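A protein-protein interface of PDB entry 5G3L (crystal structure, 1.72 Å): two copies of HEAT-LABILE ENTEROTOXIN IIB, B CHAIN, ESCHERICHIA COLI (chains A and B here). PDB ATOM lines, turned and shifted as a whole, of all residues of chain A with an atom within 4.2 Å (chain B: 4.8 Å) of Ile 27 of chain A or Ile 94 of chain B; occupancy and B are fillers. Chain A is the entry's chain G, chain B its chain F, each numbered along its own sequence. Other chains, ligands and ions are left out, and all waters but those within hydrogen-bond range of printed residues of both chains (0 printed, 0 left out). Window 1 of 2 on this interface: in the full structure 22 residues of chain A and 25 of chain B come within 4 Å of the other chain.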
ATOM      1  N   TYR A  26      -5.721  12.375  -2.614  1.00  0.00           N
ATOM      2  CA  TYR A  26      -4.624  11.861  -3.419  1.00  0.00           C
ATOM      3  C   TYR A  26      -5.164  11.545  -4.809  1.00  0.00           C
ATOM      4  O   TYR A  26      -6.147  10.817  -4.929  1.00  0.00           O
ATOM      5  CB  TYR A  26      -4.055  10.610  -2.766  1.00  0.00           C
ATOM      6  CG  TYR A  26      -2.846   9.956  -3.424  1.00  0.00           C
ATOM      7  CD1 TYR A  26      -1.666  10.687  -3.681  1.00  0.00           C
ATOM      8  CD2 TYR A  26      -2.847   8.629  -3.743  1.00  0.00           C
ATOM      9  CE1 TYR A  26      -0.567  10.100  -4.243  1.00  0.00           C
ATOM     10  CE2 TYR A  26      -1.720   8.035  -4.287  1.00  0.00           C
ATOM     11  CZ  TYR A  26      -0.586   8.770  -4.521  1.00  0.00           C
ATOM     12  OH  TYR A  26       0.559   8.185  -5.061  1.00  0.00           O
ATOM     13  N   ILE A  27      -4.525  12.127  -5.814  1.00  0.00           N
ATOM     14  CA  ILE A  27      -4.986  12.113  -7.201  1.00  0.00           C
ATOM     15  C   ILE A  27      -4.014  11.436  -8.155  1.00  0.00           C
ATOM     16  O   ILE A  27      -2.824  11.801  -8.194  1.00  0.00           O
ATOM     17  CB  ILE A  27      -5.269  13.539  -7.796  1.00  0.00           C
ATOM     18  CG1 ILE A  27      -6.353  14.258  -6.950  1.00  0.00           C
ATOM     19  CG2 ILE A  27      -5.674  13.446  -9.243  1.00  0.00           C
ATOM     20  CD1 ILE A  27      -6.433  15.770  -7.253  1.00  0.00           C
ATOM     21  N   SER A  28      -4.536  10.504  -8.950  1.00  0.00           N
ATOM     22  CA  SER A  28      -3.801   9.974 -10.107  1.00  0.00           C
ATOM     23  C   SER A  28      -4.547  10.337 -11.389  1.00  0.00           C
ATOM     24  O   SER A  28      -5.724  10.046 -11.486  1.00  0.00           O
ATOM     25  CB  SER A  28      -3.616   8.469 -10.017  1.00  0.00           C
ATOM     26  OG  SER A  28      -3.003   8.006 -11.213  1.00  0.00           O
ATOM     27  N   GLY A  36      -0.403  13.247 -14.177  1.00  0.00           N
ATOM     28  CA  GLY A  36       0.479  13.332 -13.044  1.00  0.00           C
ATOM     29  C   GLY A  36      -0.143  12.775 -11.768  1.00  0.00           C
ATOM     30  O   GLY A  36      -1.304  12.333 -11.735  1.00  0.00           O
ATOM     31  N   MET A  37       0.611  12.913 -10.691  1.00  0.00           N
ATOM     32  CA  MET A  37       0.185  12.592  -9.345  1.00  0.00           C
ATOM     33  C   MET A  37       0.159  13.870  -8.496  1.00  0.00           C
ATOM     34  O   MET A  37       1.100  14.669  -8.500  1.00  0.00           O
ATOM     35  CB  MET A  37       1.186  11.626  -8.676  1.00  0.00           C
ATOM     36  CG  MET A  37       1.342  10.302  -9.417  1.00  0.00           C
ATOM     37  SD  MET A  37      -0.169   9.368  -9.495  1.00  0.00           S
ATOM     38  CE  MET A  37      -0.694   9.360  -7.781  1.00  0.00           C
ATOM     39  N   TYR A  38      -0.912  14.044  -7.757  1.00  0.00           N
ATOM     40  CA  TYR A  38      -1.127  15.259  -6.976  1.00  0.00           C
ATOM     41  C   TYR A  38      -1.665  14.953  -5.588  1.00  0.00           C
ATOM     42  O   TYR A  38      -2.321  13.900  -5.325  1.00  0.00           O
ATOM     43  CB  TYR A  38      -2.127  16.224  -7.713  1.00  0.00           C
ATOM     44  CG  TYR A  38      -1.846  16.516  -9.128  1.00  0.00           C
ATOM     45  CD1 TYR A  38      -2.341  15.707 -10.097  1.00  0.00           C
ATOM     46  CD2 TYR A  38      -1.069  17.604  -9.510  1.00  0.00           C
ATOM     47  CE1 TYR A  38      -2.102  15.960 -11.444  1.00  0.00           C
ATOM     48  CE2 TYR A  38      -0.842  17.881 -10.830  1.00  0.00           C
ATOM     49  CZ  TYR A  38      -1.367  17.105 -11.796  1.00  0.00           C
ATOM     50  OH  TYR A  38      -1.119  17.382 -13.127  1.00  0.00           O
ATOM     51  N   VAL A  40      -3.892  17.072  -2.303  1.00  0.00           N
ATOM     52  CA  VAL A  40      -4.745  18.222  -1.913  1.00  0.00           C
ATOM     53  C   VAL A  40      -4.830  18.270  -0.383  1.00  0.00           C
ATOM     54  O   VAL A  40      -5.008  17.253   0.298  1.00  0.00           O
ATOM     55  CB  VAL A  40      -6.161  18.119  -2.470  1.00  0.00           C
ATOM     56  CG1 VAL A  40      -6.905  19.452  -2.205  1.00  0.00           C
ATOM     57  CG2 VAL A  40      -6.161  17.821  -3.942  1.00  0.00           C
ATOM     58  N   SER B   3     -12.316  17.735  -5.164  1.00  0.00           N
ATOM     59  CA  SER B   3     -11.592  19.061  -5.125  1.00  0.00           C
ATOM     60  C   SER B   3     -11.940  19.855  -6.361  1.00  0.00           C
ATOM     61  O   SER B   3     -12.211  19.301  -7.412  1.00  0.00           O
ATOM     62  CB  SER B   3     -10.090  18.832  -4.996  1.00  0.00           C
ATOM     63  OG  SER B   3      -9.556  18.182  -6.137  1.00  0.00           O
ATOM     64  N   PHE B   5      -9.820  21.368  -8.119  1.00  0.00           N
ATOM     65  CA  PHE B   5      -8.783  21.026  -9.034  1.00  0.00           C
ATOM     66  C   PHE B   5      -9.193  19.789  -9.856  1.00  0.00           C
ATOM     67  O   PHE B   5      -9.069  19.742 -11.084  1.00  0.00           O
ATOM     68  CB  PHE B   5      -7.493  20.784  -8.236  1.00  0.00           C
ATOM     69  CG  PHE B   5      -6.325  20.298  -9.051  1.00  0.00           C
ATOM     70  CD1 PHE B   5      -5.599  21.165  -9.858  1.00  0.00           C
ATOM     71  CD2 PHE B   5      -5.870  18.958  -8.909  1.00  0.00           C
ATOM     72  CE1 PHE B   5      -4.475  20.762 -10.564  1.00  0.00           C
ATOM     73  CE2 PHE B   5      -4.769  18.542  -9.650  1.00  0.00           C
ATOM     74  CZ  PHE B   5      -4.071  19.423 -10.464  1.00  0.00           C
ATOM     75  N   PHE B   6      -9.604  18.744  -9.140  1.00  0.00           N
ATOM     76  CA  PHE B   6     -10.041  17.482  -9.805  1.00  0.00           C
ATOM     77  C   PHE B   6     -11.218  17.709 -10.767  1.00  0.00           C
ATOM     78  O   PHE B   6     -11.229  17.214 -11.875  1.00  0.00           O
ATOM     79  CB  PHE B   6     -10.378  16.432  -8.746  1.00  0.00           C
ATOM     80  CG  PHE B   6     -10.591  15.042  -9.309  1.00  0.00           C
ATOM     81  CD1 PHE B   6      -9.501  14.216  -9.603  1.00  0.00           C
ATOM     82  CD2 PHE B   6     -11.836  14.591  -9.600  1.00  0.00           C
ATOM     83  CE1 PHE B   6      -9.688  12.937 -10.091  1.00  0.00           C
ATOM     84  CE2 PHE B   6     -12.046  13.336 -10.153  1.00  0.00           C
ATOM     85  CZ  PHE B   6     -10.969  12.495 -10.392  1.00  0.00           C
ATOM     86  N   MET B  64      -3.366   4.219  -9.439  1.00  0.00           N
ATOM     87  CA  MET B  64      -4.834   4.044  -9.488  1.00  0.00           C
ATOM     88  C   MET B  64      -5.208   2.723  -8.805  1.00  0.00           C
ATOM     89  O   MET B  64      -6.184   2.603  -8.089  1.00  0.00           O
ATOM     90  CB  MET B  64      -5.347   4.016 -10.944  1.00  0.00           C
ATOM     91  CG  MET B  64      -5.204   5.350 -11.628  1.00  0.00           C
ATOM     92  SD  MET B  64      -5.854   5.250 -13.289  1.00  0.00           S
ATOM     93  CE  MET B  64      -5.909   6.982 -13.855  1.00  0.00           C
ATOM     94  N   ILE B  67      -4.889   3.127  -5.067  1.00  0.00           N
ATOM     95  CA  ILE B  67      -6.050   3.902  -4.567  1.00  0.00           C
ATOM     96  C   ILE B  67      -7.257   2.950  -4.434  1.00  0.00           C
ATOM     97  O   ILE B  67      -7.990   2.966  -3.459  1.00  0.00           O
ATOM     98  CB  ILE B  67      -6.281   5.124  -5.483  1.00  0.00           C
ATOM     99  CG1 ILE B  67      -5.243   6.238  -5.188  1.00  0.00           C
ATOM    100  CG2 ILE B  67      -7.679   5.640  -5.331  1.00  0.00           C
ATOM    101  CD1 ILE B  67      -5.203   7.340  -6.236  1.00  0.00           C
ATOM    102  N   VAL B  78     -14.059   7.600  -3.188  1.00  0.00           N
ATOM    103  CA  VAL B  78     -13.306   8.130  -4.313  1.00  0.00           C
ATOM    104  C   VAL B  78     -14.205   9.038  -5.210  1.00  0.00           C
ATOM    105  O   VAL B  78     -15.430   8.876  -5.296  1.00  0.00           O
ATOM    106  CB  VAL B  78     -12.688   7.027  -5.199  1.00  0.00           C
ATOM    107  CG1 VAL B  78     -11.757   6.161  -4.342  1.00  0.00           C
ATOM    108  CG2 VAL B  78     -13.755   6.182  -5.847  1.00  0.00           C
ATOM    109  N   ASN B  79     -13.552   9.958  -5.885  1.00  0.00           N
ATOM    110  CA  ASN B  79     -14.121  10.639  -7.043  1.00  0.00           C
ATOM    111  C   ASN B  79     -13.431  10.163  -8.299  1.00  0.00           C
ATOM    112  O   ASN B  79     -12.213  10.011  -8.346  1.00  0.00           O
ATOM    113  CB  ASN B  79     -13.975  12.155  -6.855  1.00  0.00           C
ATOM    114  CG  ASN B  79     -14.404  12.561  -5.482  1.00  0.00           C
ATOM    115  OD1 ASN B  79     -15.539  12.326  -5.082  1.00  0.00           O
ATOM    116  ND2 ASN B  79     -13.482  13.122  -4.724  1.00  0.00           N
ATOM    117  N   MET B  80     -14.193   9.909  -9.367  1.00  0.00           N
ATOM    118  CA  MET B  80     -13.664   9.442 -10.592  1.00  0.00           C
ATOM    119  C   MET B  80     -13.960  10.342 -11.787  1.00  0.00           C
ATOM    120  O   MET B  80     -15.002  10.982 -11.838  1.00  0.00           O
ATOM    121  CB  MET B  80     -14.131   8.013 -10.911  1.00  0.00           C
ATOM    122  CG  MET B  80     -13.538   6.992  -9.944  1.00  0.00           C
ATOM    123  SD  MET B  80     -14.122   5.311 -10.159  1.00  0.00           S
ATOM    124  CE  MET B  80     -15.839   5.549  -9.695  1.00  0.00           C
ATOM    125  N   ILE B  91     -11.488   4.562 -16.221  1.00  0.00           N
ATOM    126  CA  ILE B  91     -11.031   5.623 -15.350  1.00  0.00           C
ATOM    127  C   ILE B  91      -9.814   6.368 -15.962  1.00  0.00           C
ATOM    128  O   ILE B  91      -8.759   5.763 -16.150  1.00  0.00           O
ATOM    129  CB  ILE B  91     -10.691   5.058 -13.951  1.00  0.00           C
ATOM    130  CG1 ILE B  91     -11.920   4.454 -13.292  1.00  0.00           C
ATOM    131  CG2 ILE B  91     -10.106   6.113 -13.029  1.00  0.00           C
ATOM    132  CD1 ILE B  91     -11.635   3.497 -12.141  1.00  0.00           C
ATOM    133  N   TRP B  92     -10.008   7.653 -16.215  1.00  0.00           N
ATOM    134  CA  TRP B  92      -8.944   8.550 -16.674  1.00  0.00           C
ATOM    135  C   TRP B  92      -8.258   9.308 -15.565  1.00  0.00           C
ATOM    136  O   TRP B  92      -7.084   9.711 -15.693  1.00  0.00           O
ATOM    137  CB  TRP B  92      -9.472   9.529 -17.724  1.00  0.00           C
ATOM    138  CG  TRP B  92      -9.736   8.897 -19.063  1.00  0.00           C
ATOM    139  CD1 TRP B  92      -9.398   7.652 -19.474  1.00  0.00           C
ATOM    140  CD2 TRP B  92     -10.419   9.521 -20.184  1.00  0.00           C
ATOM    141  NE1 TRP B  92      -9.792   7.457 -20.788  1.00  0.00           N
ATOM    142  CE2 TRP B  92     -10.422   8.591 -21.235  1.00  0.00           C
ATOM    143  CE3 TRP B  92     -10.971  10.777 -20.402  1.00  0.00           C
ATOM    144  CZ2 TRP B  92     -10.994   8.879 -22.495  1.00  0.00           C
ATOM    145  CZ3 TRP B  92     -11.553  11.050 -21.654  1.00  0.00           C
ATOM    146  CH2 TRP B  92     -11.547  10.102 -22.680  1.00  0.00           C
ATOM    147  N   ALA B  93      -8.957   9.503 -14.479  1.00  0.00           N
ATOM    148  CA  ALA B  93      -8.407  10.076 -13.243  1.00  0.00           C
ATOM    149  C   ALA B  93      -9.207   9.610 -12.047  1.00  0.00           C
ATOM    150  O   ALA B  93     -10.438   9.376 -12.121  1.00  0.00           O
ATOM    151  CB  ALA B  93      -8.399  11.614 -13.297  1.00  0.00           C
ATOM    152  N   ILE B  94      -8.547   9.549 -10.903  1.00  0.00           N
ATOM    153  CA  ILE B  94      -9.215   9.166  -9.684  1.00  0.00           C
ATOM    154  C   ILE B  94      -8.616   9.931  -8.471  1.00  0.00           C
ATOM    155  O   ILE B  94      -7.404  10.212  -8.426  1.00  0.00           O
ATOM    156  CB  ILE B  94      -9.172   7.599  -9.462  1.00  0.00           C
ATOM    157  CG1 ILE B  94     -10.016   7.140  -8.258  1.00  0.00           C
ATOM    158  CG2 ILE B  94      -7.750   7.145  -9.302  1.00  0.00           C
ATOM    159  CD1 ILE B  94     -10.308   5.646  -8.248  1.00  0.00           C
ATOM    160  N   GLU B  95      -9.474  10.220  -7.532  1.00  0.00           N
ATOM    161  CA  GLU B  95      -9.169  11.003  -6.334  1.00  0.00           C
ATOM    162  C   GLU B  95      -9.647  10.266  -5.104  1.00  0.00           C
ATOM    163  O   GLU B  95     -10.848  10.024  -4.909  1.00  0.00           O
ATOM    164  CB  GLU B  95      -9.835  12.381  -6.369  1.00  0.00           C
ATOM    165  CG  GLU B  95      -9.584  13.269  -5.130  1.00  0.00           C
ATOM    166  CD  GLU B  95     -10.087  14.708  -5.355  1.00  0.00           C
ATOM    167  OE1 GLU B  95     -11.322  14.888  -5.423  1.00  0.00           O
ATOM    168  OE2 GLU B  95      -9.249  15.650  -5.464  1.00  0.00           O
ATOM    169  N   LEU B  96      -8.702   9.844  -4.272  1.00  0.00           N
ATOM    170  CA  LEU B  96      -9.012   9.205  -2.982  1.00  0.00           C
ATOM    171  C   LEU B  96      -9.208  10.258  -1.919  1.00  0.00           C
ATOM    172  O   LEU B  96      -8.382  11.173  -1.806  1.00  0.00           O
ATOM    173  CB  LEU B  96      -7.847   8.328  -2.527  1.00  0.00           C
ATOM    174  CG  LEU B  96      -7.987   7.560  -1.210  1.00  0.00           C
ATOM    175  CD1 LEU B  96      -9.070   6.525  -1.267  1.00  0.00           C
ATOM    176  CD2 LEU B  96      -6.643   6.898  -0.878  1.00  0.00           C
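The side-chain hydroxyl (OG) of Ser 3 of chain B sits at hydrogen-bond distance from the backbone NH (N) of Phe 6 of chain B.
The side-chain hydroxyl (OG) of Ser 3 of chain B lies within hydrogen-bond range of the side-chain carboxylate (OE2) of Glu 95 of chain B (2.6 Å).
The backbone NH (N) of Glu 95 of chain B sits at hydrogen-bond distance from the backbone carbonyl oxygen (O) of Asn 79 of chain B (2.9 Å).
The backbone NH (N) of Ile 27 of chain A is in hydrogen-bond range of the backbone carbonyl oxygen (O) of Tyr 38 of chain A.
The side-chain hydroxyl of Ser 28 of chain A lies within hydrogen-bond range of the side-chain sulfur of Met 37 of chain A.
Of the 14 printed residues of chain B, 8 touch a printed residue of chain A.
Hydrophobic or aromatic side chains of chain B that line the printed part of chain A: Phe 5, Phe 6, Met 64, Ile 67, Ala 93 and Leu 96.
Along chain B the printed residues that touch a printed residue of chain A span positions 5 to 96.
Hydrophobic or aromatic side chains of chain A within 4 Å of the printed part of chain B: Tyr 26, Ile 27 and Tyr 38.
Among the printed residues, 12 pairs touch across the chains.
Among the printed residues, no Asp or Glu carboxylate lies within 4 Å of a Lys or Arg side-chain nitrogen of the other chain.
No position is printed for both chains.
Of the 12 pairs that touch across the chains among the printed residues, none has its exchanged pair printed and touching as well.
Of chain B, only Phe 5, Phe 6, Ile 94 and Glu 95 come within 4 Å of Ile 27 of chain A.
Ile 94 of chain B touches just these residues of chain A: Tyr 26 (3.8 Å), Ile 27 (3.3 Å) and Ser 28 (2.9 Å).
Of the printed residues of chain A, Ala 93 of chain B touches Ser 28.
Printed residues of chain A within 4 Å of Leu 96 of chain B: Tyr 26.
Of the printed residues of chain A, Ile 67 of chain B touches Tyr 26 (3.7 Å).
Of the printed residues of chain A, Phe 6 of chain B touches Ile 27 (3.9 Å).
The nearest residue of chain B that does not touch Ile 27 of chain A is Ser 3 of chain B (4.1 Å).
Among the printed residues, merely in contact across the chains: Tyr 26 of chain A with Ile 67 of chain B (3.7 Å), Tyr 26 of chain A with Ile 94 of chain B (3.8 Å), Tyr 26 of chain A with Glu 95 of chain B (3.3 Å), Ile 27 of chain A with Phe 5 of chain B (3.6 Å), Ile 27 of chain A with Phe 6 of chain B (3.9 Å), Ile 27 of chain A with Ile 94 of chain B (3.3 Å), Ile 27 of chain A with Glu 95 of chain B (3.3 Å), Ser 28 of chain A with Met 64 of chain B (3.5 Å), Ser 28 of chain A with Ala 93 of chain B (3.2 Å) and Tyr 38 of chain A with Phe 5 of chain B (3.6 Å).
N of Ile 94 of chain B is in hydrogen-bond range of O of Ser 28 of chain A (2.9 Å).
N of Leu 96 of chain B sits at hydrogen-bond distance from O of Tyr 26 of chain A, 2.8 Å away.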
